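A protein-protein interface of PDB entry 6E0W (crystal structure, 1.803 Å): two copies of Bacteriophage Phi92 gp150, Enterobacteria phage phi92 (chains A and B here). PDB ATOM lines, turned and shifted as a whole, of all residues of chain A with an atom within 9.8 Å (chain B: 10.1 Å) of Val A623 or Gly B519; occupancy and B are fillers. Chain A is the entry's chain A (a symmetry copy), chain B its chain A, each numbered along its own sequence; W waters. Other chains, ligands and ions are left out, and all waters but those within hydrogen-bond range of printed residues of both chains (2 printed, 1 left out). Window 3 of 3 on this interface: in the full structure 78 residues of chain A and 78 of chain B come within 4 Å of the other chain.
ND1 of His B515 is in hydrogen-bond range of NZ of Lys A521, at 2.9 Å.
N of Val A523 sits at hydrogen-bond distance from O of Val A621 (2.9 Å). O of His B515 sits at hydrogen-bond distance from N of Thr B497 (3.0 Å). The backbone carbonyl oxygen of Lys A521 sits at hydrogen-bond distance from the backbone NH of Val A623 (2.9 Å). The backbone carbonyl oxygen of Thr B497 sits at hydrogen-bond distance from the backbone NH of Ala B517, 2.9 Å away.
Among the printed residues, merely in contact across the chains: Val A513 with His B515 (3.95 Å), Val A523 with Phe B496 (3.8 Å), Thr A525 with Phe B496 (3.9 Å), Thr A525 with Ala B517 (3.9 Å), Val A621 with Ala B517 (3.4 Å) and Val A623 with Gly B519 (3.7 Å).
Val A623 touches one residue of chain B. Gly B519 touches just one residue of chain A: Val A623. Lys A521 touches just one residue of chain B: His B515. No residue of chain B comes within 4 Å of Thr A622. No residue of chain B comes within 4 Å of Asn A624. No residue of chain A comes within 4 Å of Ser B518. Printed residues of chain A within 4 Å of Phe B496: Val A523 and Thr A525. Printed residues of chain B within 4 Å of Thr A525: Phe B496 and Ala B517. Of the printed residues of chain A, His B515 touches Val A513 and Lys A521. Of the printed residues of chain B, Val A621 touches Ala B517 (3.4 Å). Ser A518 touches none of the printed residues of chain B. Thr B497 touches none of the printed residues of chain A. The nearest residue of chain B that does not touch Val A623 is Asn B624 (4.6 Å). The nearest residue of chain A that does not touch Gly B519 is Lys A521 (4.3 Å). The nearest printed residue of chain B that does not touch Val A523 is Cys B516 (4.4 Å).
Hydrophobic or aromatic side chains of chain A within 4 Å of the printed part of chain B: Val A513, Val A523, Val A621 and Val A623. Of the 19 printed residues of chain B, 4 touch a printed residue of chain A.
Val A513 touches His B515, but with the chains exchanged His A515 does not touch Val B513 (7.4 Å). Lys A521 touches His B515, but with the chains exchanged His A515 does not touch Lys B521 (6.6 Å). Val A623 touches Gly B519, but with the chains exchanged Gly A519 does not touch Val B623 (9.9 Å).
Water W1 bridges a ring nitrogen (NE2) of His A515 (3.1 Å) and a ring nitrogen (NE2) of His B515 (3.1 Å). Water W2 bridges NZ of Lys A521 and NZ of Lys B521.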
ATOM      1  N   ASP A 500      36.153  19.495 -14.428  1.00  0.00           N
ATOM      2  CA  ASP A 500      35.892  19.227 -15.842  1.00  0.00           C
ATOM      3  C   ASP A 500      34.877  18.135 -16.081  1.00  0.00           C
ATOM      4  O   ASP A 500      34.215  18.169 -17.119  1.00  0.00           O
ATOM      5  CB  ASP A 500      37.179  18.841 -16.567  1.00  0.00           C
ATOM      6  CG  ASP A 500      38.067  20.055 -16.881  1.00  0.00           C
ATOM      7  OD1 ASP A 500      37.643  21.220 -16.679  1.00  0.00           O
ATOM      8  OD2 ASP A 500      39.188  19.822 -17.347  1.00  0.00           O
ATOM      9  N   PHE A 502      31.600  15.923 -16.363  1.00  0.00           N
ATOM     10  CA  PHE A 502      30.207  16.334 -16.424  1.00  0.00           C
ATOM     11  C   PHE A 502      29.519  16.025 -15.086  1.00  0.00           C
ATOM     12  O   PHE A 502      29.734  14.951 -14.513  1.00  0.00           O
ATOM     13  CB  PHE A 502      29.505  15.615 -17.597  1.00  0.00           C
ATOM     14  CG  PHE A 502      28.140  16.149 -17.877  1.00  0.00           C
ATOM     15  CD1 PHE A 502      27.968  17.277 -18.710  1.00  0.00           C
ATOM     16  CD2 PHE A 502      27.030  15.606 -17.245  1.00  0.00           C
ATOM     17  CE1 PHE A 502      26.682  17.783 -18.941  1.00  0.00           C
ATOM     18  CE2 PHE A 502      25.757  16.103 -17.467  1.00  0.00           C
ATOM     19  CZ  PHE A 502      25.582  17.202 -18.336  1.00  0.00           C
ATOM     20  N   VAL A 513      24.034  24.676 -20.817  1.00  0.00           N
ATOM     21  CA  VAL A 513      25.474  24.871 -20.980  1.00  0.00           C
ATOM     22  C   VAL A 513      26.149  24.802 -19.615  1.00  0.00           C
ATOM     23  O   VAL A 513      25.712  25.465 -18.670  1.00  0.00           O
ATOM     24  CB  VAL A 513      25.805  26.222 -21.633  1.00  0.00           C
ATOM     25  CG1 VAL A 513      27.351  26.366 -21.815  1.00  0.00           C
ATOM     26  CG2 VAL A 513      25.097  26.308 -22.968  1.00  0.00           C
ATOM     27  N   ILE A 514      27.216  24.023 -19.523  1.00  0.00           N
ATOM     28  CA  ILE A 514      28.037  23.963 -18.304  1.00  0.00           C
ATOM     29  C   ILE A 514      29.389  24.569 -18.646  1.00  0.00           C
ATOM     30  O   ILE A 514      30.072  24.060 -19.550  1.00  0.00           O
ATOM     31  CB  ILE A 514      28.236  22.523 -17.794  1.00  0.00           C
ATOM     32  CG1 ILE A 514      26.934  21.701 -17.696  1.00  0.00           C
ATOM     33  CG2 ILE A 514      29.020  22.552 -16.422  1.00  0.00           C
ATOM     34  CD1 ILE A 514      25.883  22.332 -16.817  1.00  0.00           C
ATOM     35  N   HIS A 515      29.799  25.626 -17.913  1.00  0.00           N
ATOM     36  CA  HIS A 515      31.092  26.287 -18.118  1.00  0.00           C
ATOM     37  C   HIS A 515      32.062  25.800 -17.049  1.00  0.00           C
ATOM     38  O   HIS A 515      31.776  25.934 -15.861  1.00  0.00           O
ATOM     39  CB  HIS A 515      30.965  27.813 -18.020  1.00  0.00           C
ATOM     40  CG  HIS A 515      30.101  28.401 -19.103  1.00  0.00           C
ATOM     41  ND1 HIS A 515      30.608  28.826 -20.313  1.00  0.00           N
ATOM     42  CD2 HIS A 515      28.765  28.634 -19.154  1.00  0.00           C
ATOM     43  CE1 HIS A 515      29.621  29.302 -21.067  1.00  0.00           C
ATOM     44  NE2 HIS A 515      28.493  29.198 -20.382  1.00  0.00           N
ATOM     45  N   CYS A 516      33.203  25.266 -17.472  1.00  0.00           N
ATOM     46  CA  CYS A 516      34.202  24.722 -16.540  1.00  0.00           C
ATOM     47  C   CYS A 516      35.256  25.771 -16.201  1.00  0.00           C
ATOM     48  O   CYS A 516      35.597  26.647 -17.022  1.00  0.00           O
ATOM     49  CB  CYS A 516      34.880  23.492 -17.124  1.00  0.00           C
ATOM     50  SG  CYS A 516      33.678  22.214 -17.620  1.00  0.00           S
ATOM     51  N   SER A 518      38.264  25.384 -16.099  1.00  0.00           N
ATOM     52  CA  SER A 518      39.406  25.232 -16.999  1.00  0.00           C
ATOM     53  C   SER A 518      39.209  25.953 -18.319  1.00  0.00           C
ATOM     54  O   SER A 518      40.155  26.034 -19.105  1.00  0.00           O
ATOM     55  CB  SER A 518      39.645  23.779 -17.328  1.00  0.00           C
ATOM     56  OG  SER A 518      38.491  23.329 -18.022  1.00  0.00           O
ATOM     57  N   GLY A 519      38.005  26.403 -18.610  1.00  0.00           N
ATOM     58  CA  GLY A 519      37.675  26.930 -19.909  1.00  0.00           C
ATOM     59  C   GLY A 519      36.901  25.975 -20.797  1.00  0.00           C
ATOM     60  O   GLY A 519      36.334  26.425 -21.797  1.00  0.00           O
ATOM     61  N   LYS A 520      36.888  24.676 -20.485  1.00  0.00           N
ATOM     62  CA  LYS A 520      36.048  23.734 -21.215  1.00  0.00           C
ATOM     63  C   LYS A 520      34.579  24.113 -21.047  1.00  0.00           C
ATOM     64  O   LYS A 520      34.222  24.884 -20.169  1.00  0.00           O
ATOM     65  CB  LYS A 520      36.252  22.305 -20.722  1.00  0.00           C
ATOM     66  CG  LYS A 520      37.607  21.711 -21.010  1.00  0.00           C
ATOM     67  CD  LYS A 520      37.620  20.180 -20.685  1.00  0.00           C
ATOM     68  CE  LYS A 520      39.051  19.664 -20.692  1.00  0.00           C
ATOM     69  NZ  LYS A 520      40.012  20.633 -20.012  1.00  0.00           N
ATOM     70  N   LYS A 521      33.723  23.593 -21.924  1.00  0.00           N
ATOM     71  CA  LYS A 521      32.288  23.792 -21.744  1.00  0.00           C
ATOM     72  C   LYS A 521      31.581  22.548 -22.249  1.00  0.00           C
ATOM     73  O   LYS A 521      32.067  21.891 -23.161  1.00  0.00           O
ATOM     74  CB  LYS A 521      31.725  25.021 -22.472  1.00  0.00           C
ATOM     75  CG  LYS A 521      31.592  24.957 -23.920  1.00  0.00           C
ATOM     76  CD  LYS A 521      30.609  26.068 -24.397  1.00  0.00           C
ATOM     77  CE  LYS A 521      30.504  26.114 -25.909  1.00  0.00           C
ATOM     78  NZ  LYS A 521      29.584  27.187 -26.452  1.00  0.00           N
ATOM     79  N   HIS A 522      30.486  22.194 -21.598  1.00  0.00           N
ATOM     80  CA  HIS A 522      29.626  21.110 -22.034  1.00  0.00           C
ATOM     81  C   HIS A 522      28.339  21.744 -22.533  1.00  0.00           C
ATOM     82  O   HIS A 522      27.820  22.671 -21.911  1.00  0.00           O
ATOM     83  CB  HIS A 522      29.308  20.116 -20.902  1.00  0.00           C
ATOM     84  CG  HIS A 522      30.513  19.619 -20.170  1.00  0.00           C
ATOM     85  ND1 HIS A 522      31.422  18.748 -20.742  1.00  0.00           N
ATOM     86  CD2 HIS A 522      30.943  19.835 -18.900  1.00  0.00           C
ATOM     87  CE1 HIS A 522      32.369  18.465 -19.855  1.00  0.00           C
ATOM     88  NE2 HIS A 522      32.107  19.120 -18.735  1.00  0.00           N
ATOM     89  N   VAL A 523      27.824  21.238 -23.642  1.00  0.00           N
ATOM     90  CA  VAL A 523      26.525  21.648 -24.158  1.00  0.00           C
ATOM     91  C   VAL A 523      25.615  20.427 -24.186  1.00  0.00           C
ATOM     92  O   VAL A 523      25.956  19.409 -24.794  1.00  0.00           O
ATOM     93  CB  VAL A 523      26.648  22.266 -25.558  1.00  0.00           C
ATOM     94  CG1 VAL A 523      25.258  22.625 -26.089  1.00  0.00           C
ATOM     95  CG2 VAL A 523      27.592  23.515 -25.505  1.00  0.00           C
ATOM     96  N   VAL A 524      24.473  20.522 -23.515  1.00  0.00           N
ATOM     97  CA  VAL A 524      23.549  19.393 -23.443  1.00  0.00           C
ATOM     98  C   VAL A 524      22.732  19.385 -24.730  1.00  0.00           C
ATOM     99  O   VAL A 524      21.947  20.308 -24.967  1.00  0.00           O
ATOM    100  CB  VAL A 524      22.637  19.486 -22.219  1.00  0.00           C
ATOM    101  CG1 VAL A 524      21.608  18.341 -22.277  1.00  0.00           C
ATOM    102  CG2 VAL A 524      23.483  19.373 -20.908  1.00  0.00           C
ATOM    103  N   THR A 525      22.922  18.350 -25.559  1.00  0.00           N
ATOM    104  CA  THR A 525      22.211  18.239 -26.837  1.00  0.00           C
ATOM    105  C   THR A 525      20.982  17.350 -26.743  1.00  0.00           C
ATOM    106  O   THR A 525      20.098  17.471 -27.598  1.00  0.00           O
ATOM    107  CB  THR A 525      23.136  17.708 -27.939  1.00  0.00           C
ATOM    108  OG1 THR A 525      23.618  16.414 -27.570  1.00  0.00           O
ATOM    109  CG2 THR A 525      24.341  18.637 -28.144  1.00  0.00           C
ATOM    110  N   PHE A 620      25.630  15.000 -24.209  1.00  0.00           N
ATOM    111  CA  PHE A 620      26.260  16.311 -24.228  1.00  0.00           C
ATOM    112  C   PHE A 620      27.491  16.249 -25.117  1.00  0.00           C
ATOM    113  O   PHE A 620      28.016  15.168 -25.376  1.00  0.00           O
ATOM    114  CB  PHE A 620      26.630  16.807 -22.811  1.00  0.00           C
ATOM    115  CG  PHE A 620      27.609  15.904 -22.058  1.00  0.00           C
ATOM    116  CD1 PHE A 620      28.998  16.096 -22.164  1.00  0.00           C
ATOM    117  CD2 PHE A 620      27.133  14.870 -21.244  1.00  0.00           C
ATOM    118  CE1 PHE A 620      29.903  15.270 -21.468  1.00  0.00           C
ATOM    119  CE2 PHE A 620      28.049  14.019 -20.508  1.00  0.00           C
ATOM    120  CZ  PHE A 620      29.424  14.221 -20.639  1.00  0.00           C
ATOM    121  N   VAL A 621      27.935  17.420 -25.620  1.00  0.00           N
ATOM    122  CA  VAL A 621      29.217  17.525 -26.307  1.00  0.00           C
ATOM    123  C   VAL A 621      30.098  18.424 -25.451  1.00  0.00           C
ATOM    124  O   VAL A 621      29.607  19.262 -24.688  1.00  0.00           O
ATOM    125  CB  VAL A 621      29.135  18.060 -27.761  1.00  0.00           C
ATOM    126  CG1 VAL A 621      28.342  17.113 -28.649  1.00  0.00           C
ATOM    127  CG2 VAL A 621      28.541  19.437 -27.813  1.00  0.00           C
ATOM    128  N   THR A 622      31.406  18.243 -25.568  1.00  0.00           N
ATOM    129  CA  THR A 622      32.374  19.023 -24.801  1.00  0.00           C
ATOM    130  C   THR A 622      33.284  19.798 -25.755  1.00  0.00           C
ATOM    131  O   THR A 622      33.812  19.225 -26.708  1.00  0.00           O
ATOM    132  CB  THR A 622      33.176  18.096 -23.874  1.00  0.00           C
ATOM    133  OG1 THR A 622      32.267  17.435 -22.968  1.00  0.00           O
ATOM    134  CG2 THR A 622      34.217  18.899 -23.054  1.00  0.00           C
ATOM    135  N   VAL A 623      33.431  21.101 -25.536  1.00  0.00           N
ATOM    136  CA  VAL A 623      34.323  21.943 -26.340  1.00  0.00           C
ATOM    137  C   VAL A 623      35.564  22.190 -25.482  1.00  0.00           C
ATOM    138  O   VAL A 623      35.442  22.672 -24.348  1.00  0.00           O
ATOM    139  CB  VAL A 623      33.629  23.255 -26.751  1.00  0.00           C
ATOM    140  CG1 VAL A 623      34.584  24.208 -27.474  1.00  0.00           C
ATOM    141  CG2 VAL A 623      32.421  22.963 -27.633  1.00  0.00           C
ATOM    142  N   ASN A 624      36.740  21.843 -26.037  1.00  0.00           N
ATOM    143  CA  ASN A 624      38.078  21.735 -25.378  1.00  0.00           C
ATOM    144  C   ASN A 624      38.239  20.528 -24.424  1.00  0.00           C
ATOM    145  O   ASN A 624      38.184  19.351 -24.818  1.00  0.00           O
ATOM    146  CB  ASN A 624      38.465  22.987 -24.594  1.00  0.00           C
ATOM    147  CG  ASN A 624      39.056  24.009 -25.457  1.00  0.00           C
ATOM    148  OD1 ASN A 624      39.295  23.736 -26.639  1.00  0.00           O
ATOM    149  ND2 ASN A 624      39.455  25.152 -24.868  1.00  0.00           N
ATOM    150  N   PHE B 496      19.781  27.541 -28.069  1.00  0.00           N
ATOM    151  CA  PHE B 496      20.470  26.377 -28.589  1.00  0.00           C
ATOM    152  C   PHE B 496      19.842  25.990 -29.917  1.00  0.00           C
ATOM    153  O   PHE B 496      18.622  26.021 -30.043  1.00  0.00           O
ATOM    154  CB  PHE B 496      20.328  25.205 -27.567  1.00  0.00           C
ATOM    155  CG  PHE B 496      20.721  23.858 -28.106  1.00  0.00           C
ATOM    156  CD1 PHE B 496      22.066  23.464 -28.110  1.00  0.00           C
ATOM    157  CD2 PHE B 496      19.754  22.950 -28.558  1.00  0.00           C
ATOM    158  CE1 PHE B 496      22.455  22.198 -28.606  1.00  0.00           C
ATOM    159  CE2 PHE B 496      20.130  21.682 -29.051  1.00  0.00           C
ATOM    160  CZ  PHE B 496      21.482  21.307 -29.075  1.00  0.00           C
ATOM    161  N   THR B 497      20.666  25.652 -30.910  1.00  0.00           N
ATOM    162  CA  THR B 497      20.166  25.119 -32.168  1.00  0.00           C
ATOM    163  C   THR B 497      20.813  23.775 -32.460  1.00  0.00           C
ATOM    164  O   THR B 497      22.009  23.570 -32.213  1.00  0.00           O
ATOM    165  CB  THR B 497      20.419  26.114 -33.335  1.00  0.00           C
ATOM    166  OG1 THR B 497      21.818  26.392 -33.467  1.00  0.00           O
ATOM    167  CG2 THR B 497      19.700  27.390 -33.095  1.00  0.00           C
ATOM    168  N   ALA B 498      20.022  22.836 -32.976  1.00  0.00           N
ATOM    169  CA  ALA B 498      20.648  21.576 -33.356  1.00  0.00           C
ATOM    170  C   ALA B 498      21.468  21.694 -34.663  1.00  0.00           C
ATOM    171  O   ALA B 498      22.176  20.758 -35.034  1.00  0.00           O
ATOM    172  CB  ALA B 498      19.570  20.497 -33.485  1.00  0.00           C
ATOM    173  N   TYR B 499      21.508  22.858 -35.282  1.00  0.00           N
ATOM    174  CA  TYR B 499      22.143  23.051 -36.579  1.00  0.00           C
ATOM    175  C   TYR B 499      23.156  24.190 -36.465  1.00  0.00           C
ATOM    176  O   TYR B 499      23.171  24.945 -35.478  1.00  0.00           O
ATOM    177  CB  TYR B 499      21.072  23.355 -37.651  1.00  0.00           C
ATOM    178  CG  TYR B 499      20.092  24.428 -37.204  1.00  0.00           C
ATOM    179  CD1 TYR B 499      20.382  25.800 -37.389  1.00  0.00           C
ATOM    180  CD2 TYR B 499      18.888  24.085 -36.596  1.00  0.00           C
ATOM    181  CE1 TYR B 499      19.514  26.781 -36.951  1.00  0.00           C
ATOM    182  CE2 TYR B 499      17.994  25.089 -36.154  1.00  0.00           C
ATOM    183  CZ  TYR B 499      18.334  26.426 -36.334  1.00  0.00           C
ATOM    184  OH  TYR B 499      17.474  27.422 -35.882  1.00  0.00           O
ATOM    185  N   ASP B 500      24.011  24.319 -37.484  1.00  0.00           N
ATOM    186  CA  ASP B 500      25.077  25.321 -37.448  1.00  0.00           C
ATOM    187  C   ASP B 500      24.696  26.643 -38.071  1.00  0.00           C
ATOM    188  O   ASP B 500      25.256  27.662 -37.666  1.00  0.00           O
ATOM    189  CB  ASP B 500      26.326  24.807 -38.160  1.00  0.00           C
ATOM    190  CG  ASP B 500      27.127  23.812 -37.304  1.00  0.00           C
ATOM    191  OD1 ASP B 500      26.815  23.614 -36.103  1.00  0.00           O
ATOM    192  OD2 ASP B 500      28.079  23.246 -37.851  1.00  0.00           O
ATOM    193  N   VAL B 513      23.709  35.089 -27.561  1.00  0.00           N
ATOM    194  CA  VAL B 513      24.591  33.962 -27.864  1.00  0.00           C
ATOM    195  C   VAL B 513      23.756  32.785 -28.350  1.00  0.00           C
ATOM    196  O   VAL B 513      22.766  32.418 -27.710  1.00  0.00           O
ATOM    197  CB  VAL B 513      25.410  33.524 -26.640  1.00  0.00           C
ATOM    198  CG1 VAL B 513      26.359  32.342 -27.025  1.00  0.00           C
ATOM    199  CG2 VAL B 513      26.205  34.706 -26.130  1.00  0.00           C
ATOM    200  N   ILE B 514      24.165  32.187 -29.459  1.00  0.00           N
ATOM    201  CA  ILE B 514      23.529  30.963 -29.968  1.00  0.00           C
ATOM    202  C   ILE B 514      24.547  29.843 -29.835  1.00  0.00           C
ATOM    203  O   ILE B 514      25.637  29.938 -30.423  1.00  0.00           O
ATOM    204  CB  ILE B 514      23.095  31.090 -31.442  1.00  0.00           C
ATOM    205  CG1 ILE B 514      22.298  32.372 -31.759  1.00  0.00           C
ATOM    206  CG2 ILE B 514      22.315  29.786 -31.876  1.00  0.00           C
ATOM    207  CD1 ILE B 514      21.052  32.531 -30.924  1.00  0.00           C
ATOM    208  N   HIS B 515      24.194  28.767 -29.099  1.00  0.00           N
ATOM    209  CA  HIS B 515      25.069  27.604 -28.913  1.00  0.00           C
ATOM    210  C   HIS B 515      24.609  26.495 -29.850  1.00  0.00           C
ATOM    211  O   HIS B 515      23.452  26.085 -29.787  1.00  0.00           O
ATOM    212  CB  HIS B 515      25.021  27.091 -27.469  1.00  0.00           C
ATOM    213  CG  HIS B 515      25.554  28.087 -26.473  1.00  0.00           C
ATOM    214  ND1 HIS B 515      26.879  28.125 -26.093  1.00  0.00           N
ATOM    215  CD2 HIS B 515      24.936  29.077 -25.782  1.00  0.00           C
ATOM    216  CE1 HIS B 515      27.059  29.097 -25.204  1.00  0.00           C
ATOM    217  NE2 HIS B 515      25.891  29.686 -24.996  1.00  0.00           N
ATOM    218  N   CYS B 516      25.516  26.003 -30.688  1.00  0.00           N
ATOM    219  CA  CYS B 516      25.184  24.959 -31.669  1.00  0.00           C
ATOM    220  C   CYS B 516      25.496  23.573 -31.114  1.00  0.00           C
ATOM    221  O   CYS B 516      26.432  23.384 -30.310  1.00  0.00           O
ATOM    222  CB  CYS B 516      25.948  25.168 -32.968  1.00  0.00           C
ATOM    223  SG  CYS B 516      25.682  26.832 -33.662  1.00  0.00           S
ATOM    224  N   ALA B 517      24.712  22.590 -31.562  1.00  0.00           N
ATOM    225  CA  ALA B 517      24.940  21.233 -31.088  1.00  0.00           C
ATOM    226  C   ALA B 517      26.334  20.754 -31.463  1.00  0.00           C
ATOM    227  O   ALA B 517      26.877  19.867 -30.798  1.00  0.00           O
ATOM    228  CB  ALA B 517      23.883  20.278 -31.659  1.00  0.00           C
ATOM    229  N   SER B 518      26.906  21.296 -32.542  1.00  0.00           N
ATOM    230  CA  SER B 518      28.247  20.898 -32.962  1.00  0.00           C
ATOM    231  C   SER B 518      29.331  21.436 -32.046  1.00  0.00           C
ATOM    232  O   SER B 518      30.491  21.046 -32.196  1.00  0.00           O
ATOM    233  CB  SER B 518      28.556  21.410 -34.347  1.00  0.00           C
ATOM    234  OG  SER B 518      28.538  22.827 -34.265  1.00  0.00           O
ATOM    235  N   GLY B 519      29.000  22.360 -31.167  1.00  0.00           N
ATOM    236  CA  GLY B 519      29.985  23.064 -30.386  1.00  0.00           C
ATOM    237  C   GLY B 519      30.293  24.464 -30.879  1.00  0.00           C
ATOM    238  O   GLY B 519      30.896  25.236 -30.128  1.00  0.00           O
ATOM    239  N   LYS B 520      29.933  24.803 -32.120  1.00  0.00           N
ATOM    240  CA  LYS B 520      30.073  26.172 -32.598  1.00  0.00           C
ATOM    241  C   LYS B 520      29.210  27.106 -31.755  1.00  0.00           C
ATOM    242  O   LYS B 520      28.325  26.669 -31.034  1.00  0.00           O
ATOM    243  CB  LYS B 520      29.658  26.300 -34.061  1.00  0.00           C
ATOM    244  CG  LYS B 520      30.553  25.594 -35.048  1.00  0.00           C
ATOM    245  CD  LYS B 520      30.179  25.990 -36.516  1.00  0.00           C
ATOM    246  CE  LYS B 520      30.876  25.059 -37.495  1.00  0.00           C
ATOM    247  NZ  LYS B 520      30.841  23.608 -37.027  1.00  0.00           N
ATOM    248  N   LYS B 521      29.496  28.405 -31.817  1.00  0.00           N
ATOM    249  CA  LYS B 521      28.627  29.373 -31.152  1.00  0.00           C
ATOM    250  C   LYS B 521      28.622  30.639 -31.989  1.00  0.00           C
ATOM    251  O   LYS B 521      29.609  30.949 -32.644  1.00  0.00           O
ATOM    252  CB  LYS B 521      29.050  29.719 -29.717  1.00  0.00           C
ATOM    253  CG  LYS B 521      30.224  30.560 -29.534  1.00  0.00           C
ATOM    254  CD  LYS B 521      30.208  31.157 -28.094  1.00  0.00           C
ATOM    255  CE  LYS B 521      31.459  31.967 -27.810  1.00  0.00           C
ATOM    256  NZ  LYS B 521      31.530  32.562 -26.419  1.00  0.00           N
ATOM    257  N   HIS B 522      27.484  31.312 -32.020  1.00  0.00           N
ATOM    258  CA  HIS B 522      27.352  32.606 -32.664  1.00  0.00           C
ATOM    259  C   HIS B 522      27.171  33.630 -31.556  1.00  0.00           C
ATOM    260  O   HIS B 522      26.435  33.389 -30.599  1.00  0.00           O
ATOM    261  CB  HIS B 522      26.152  32.667 -33.626  1.00  0.00           C
ATOM    262  CG  HIS B 522      26.100  31.543 -34.609  1.00  0.00           C
ATOM    263  ND1 HIS B 522      26.994  31.431 -35.658  1.00  0.00           N
ATOM    264  CD2 HIS B 522      25.240  30.498 -34.732  1.00  0.00           C
ATOM    265  CE1 HIS B 522      26.693  30.353 -36.373  1.00  0.00           C
ATOM    266  NE2 HIS B 522      25.640  29.766 -35.826  1.00  0.00           N
ATOM    267  N   VAL B 523      27.830  34.769 -31.693  1.00  0.00           N
ATOM    268  CA  VAL B 523      27.643  35.894 -30.787  1.00  0.00           C
ATOM    269  C   VAL B 523      27.126  37.077 -31.595  1.00  0.00           C
ATOM    270  O   VAL B 523      27.754  37.485 -32.575  1.00  0.00           O
ATOM    271  CB  VAL B 523      28.950  36.258 -30.068  1.00  0.00           C
ATOM    272  CG1 VAL B 523      28.726  37.481 -29.176  1.00  0.00           C
ATOM    273  CG2 VAL B 523      29.465  35.025 -29.250  1.00  0.00           C
ATOM    274  N   THR B 622      31.102  34.006 -35.465  1.00  0.00           N
ATOM    275  CA  THR B 622      30.985  32.578 -35.186  1.00  0.00           C
ATOM    276  C   THR B 622      32.317  32.043 -34.658  1.00  0.00           C
ATOM    277  O   THR B 622      33.366  32.310 -35.246  1.00  0.00           O
ATOM    278  CB  THR B 622      30.533  31.834 -36.452  1.00  0.00           C
ATOM    279  OG1 THR B 622      29.249  32.348 -36.869  1.00  0.00           O
ATOM    280  CG2 THR B 622      30.408  30.312 -36.185  1.00  0.00           C
ATOM    281  N   VAL B 623      32.289  31.336 -33.533  1.00  0.00           N
ATOM    282  CA  VAL B 623      33.488  30.718 -32.956  1.00  0.00           C
ATOM    283  C   VAL B 623      33.395  29.227 -33.280  1.00  0.00           C
ATOM    284  O   VAL B 623      32.390  28.586 -32.945  1.00  0.00           O
ATOM    285  CB  VAL B 623      33.576  30.980 -31.442  1.00  0.00           C
ATOM    286  CG1 VAL B 623      34.745  30.231 -30.795  1.00  0.00           C
ATOM    287  CG2 VAL B 623      33.704  32.475 -31.168  1.00  0.00           C
ATOM    288  N   ASN B 624      34.444  28.702 -33.940  1.00  0.00           N
ATOM    289  CA  ASN B 624      34.549  27.364 -34.598  1.00  0.00           C
ATOM    290  C   ASN B 624      33.730  27.215 -35.903  1.00  0.00           C
ATOM    291  O   ASN B 624      33.963  27.889 -36.920  1.00  0.00           O
ATOM    292  CB  ASN B 624      34.153  26.210 -33.682  1.00  0.00           C
ATOM    293  CG  ASN B 624      35.262  25.790 -32.824  1.00  0.00           C
ATOM    294  OD1 ASN B 624      36.381  26.285 -33.002  1.00  0.00           O
ATOM    295  ND2 ASN B 624      35.032  24.762 -31.987  1.00  0.00           N
HETATM  296  O   HOH W   1      27.119  31.095 -22.472  1.00  0.00           O
HETATM  297  O   HOH W   2      30.695  29.813 -24.624  1.00  0.00           O
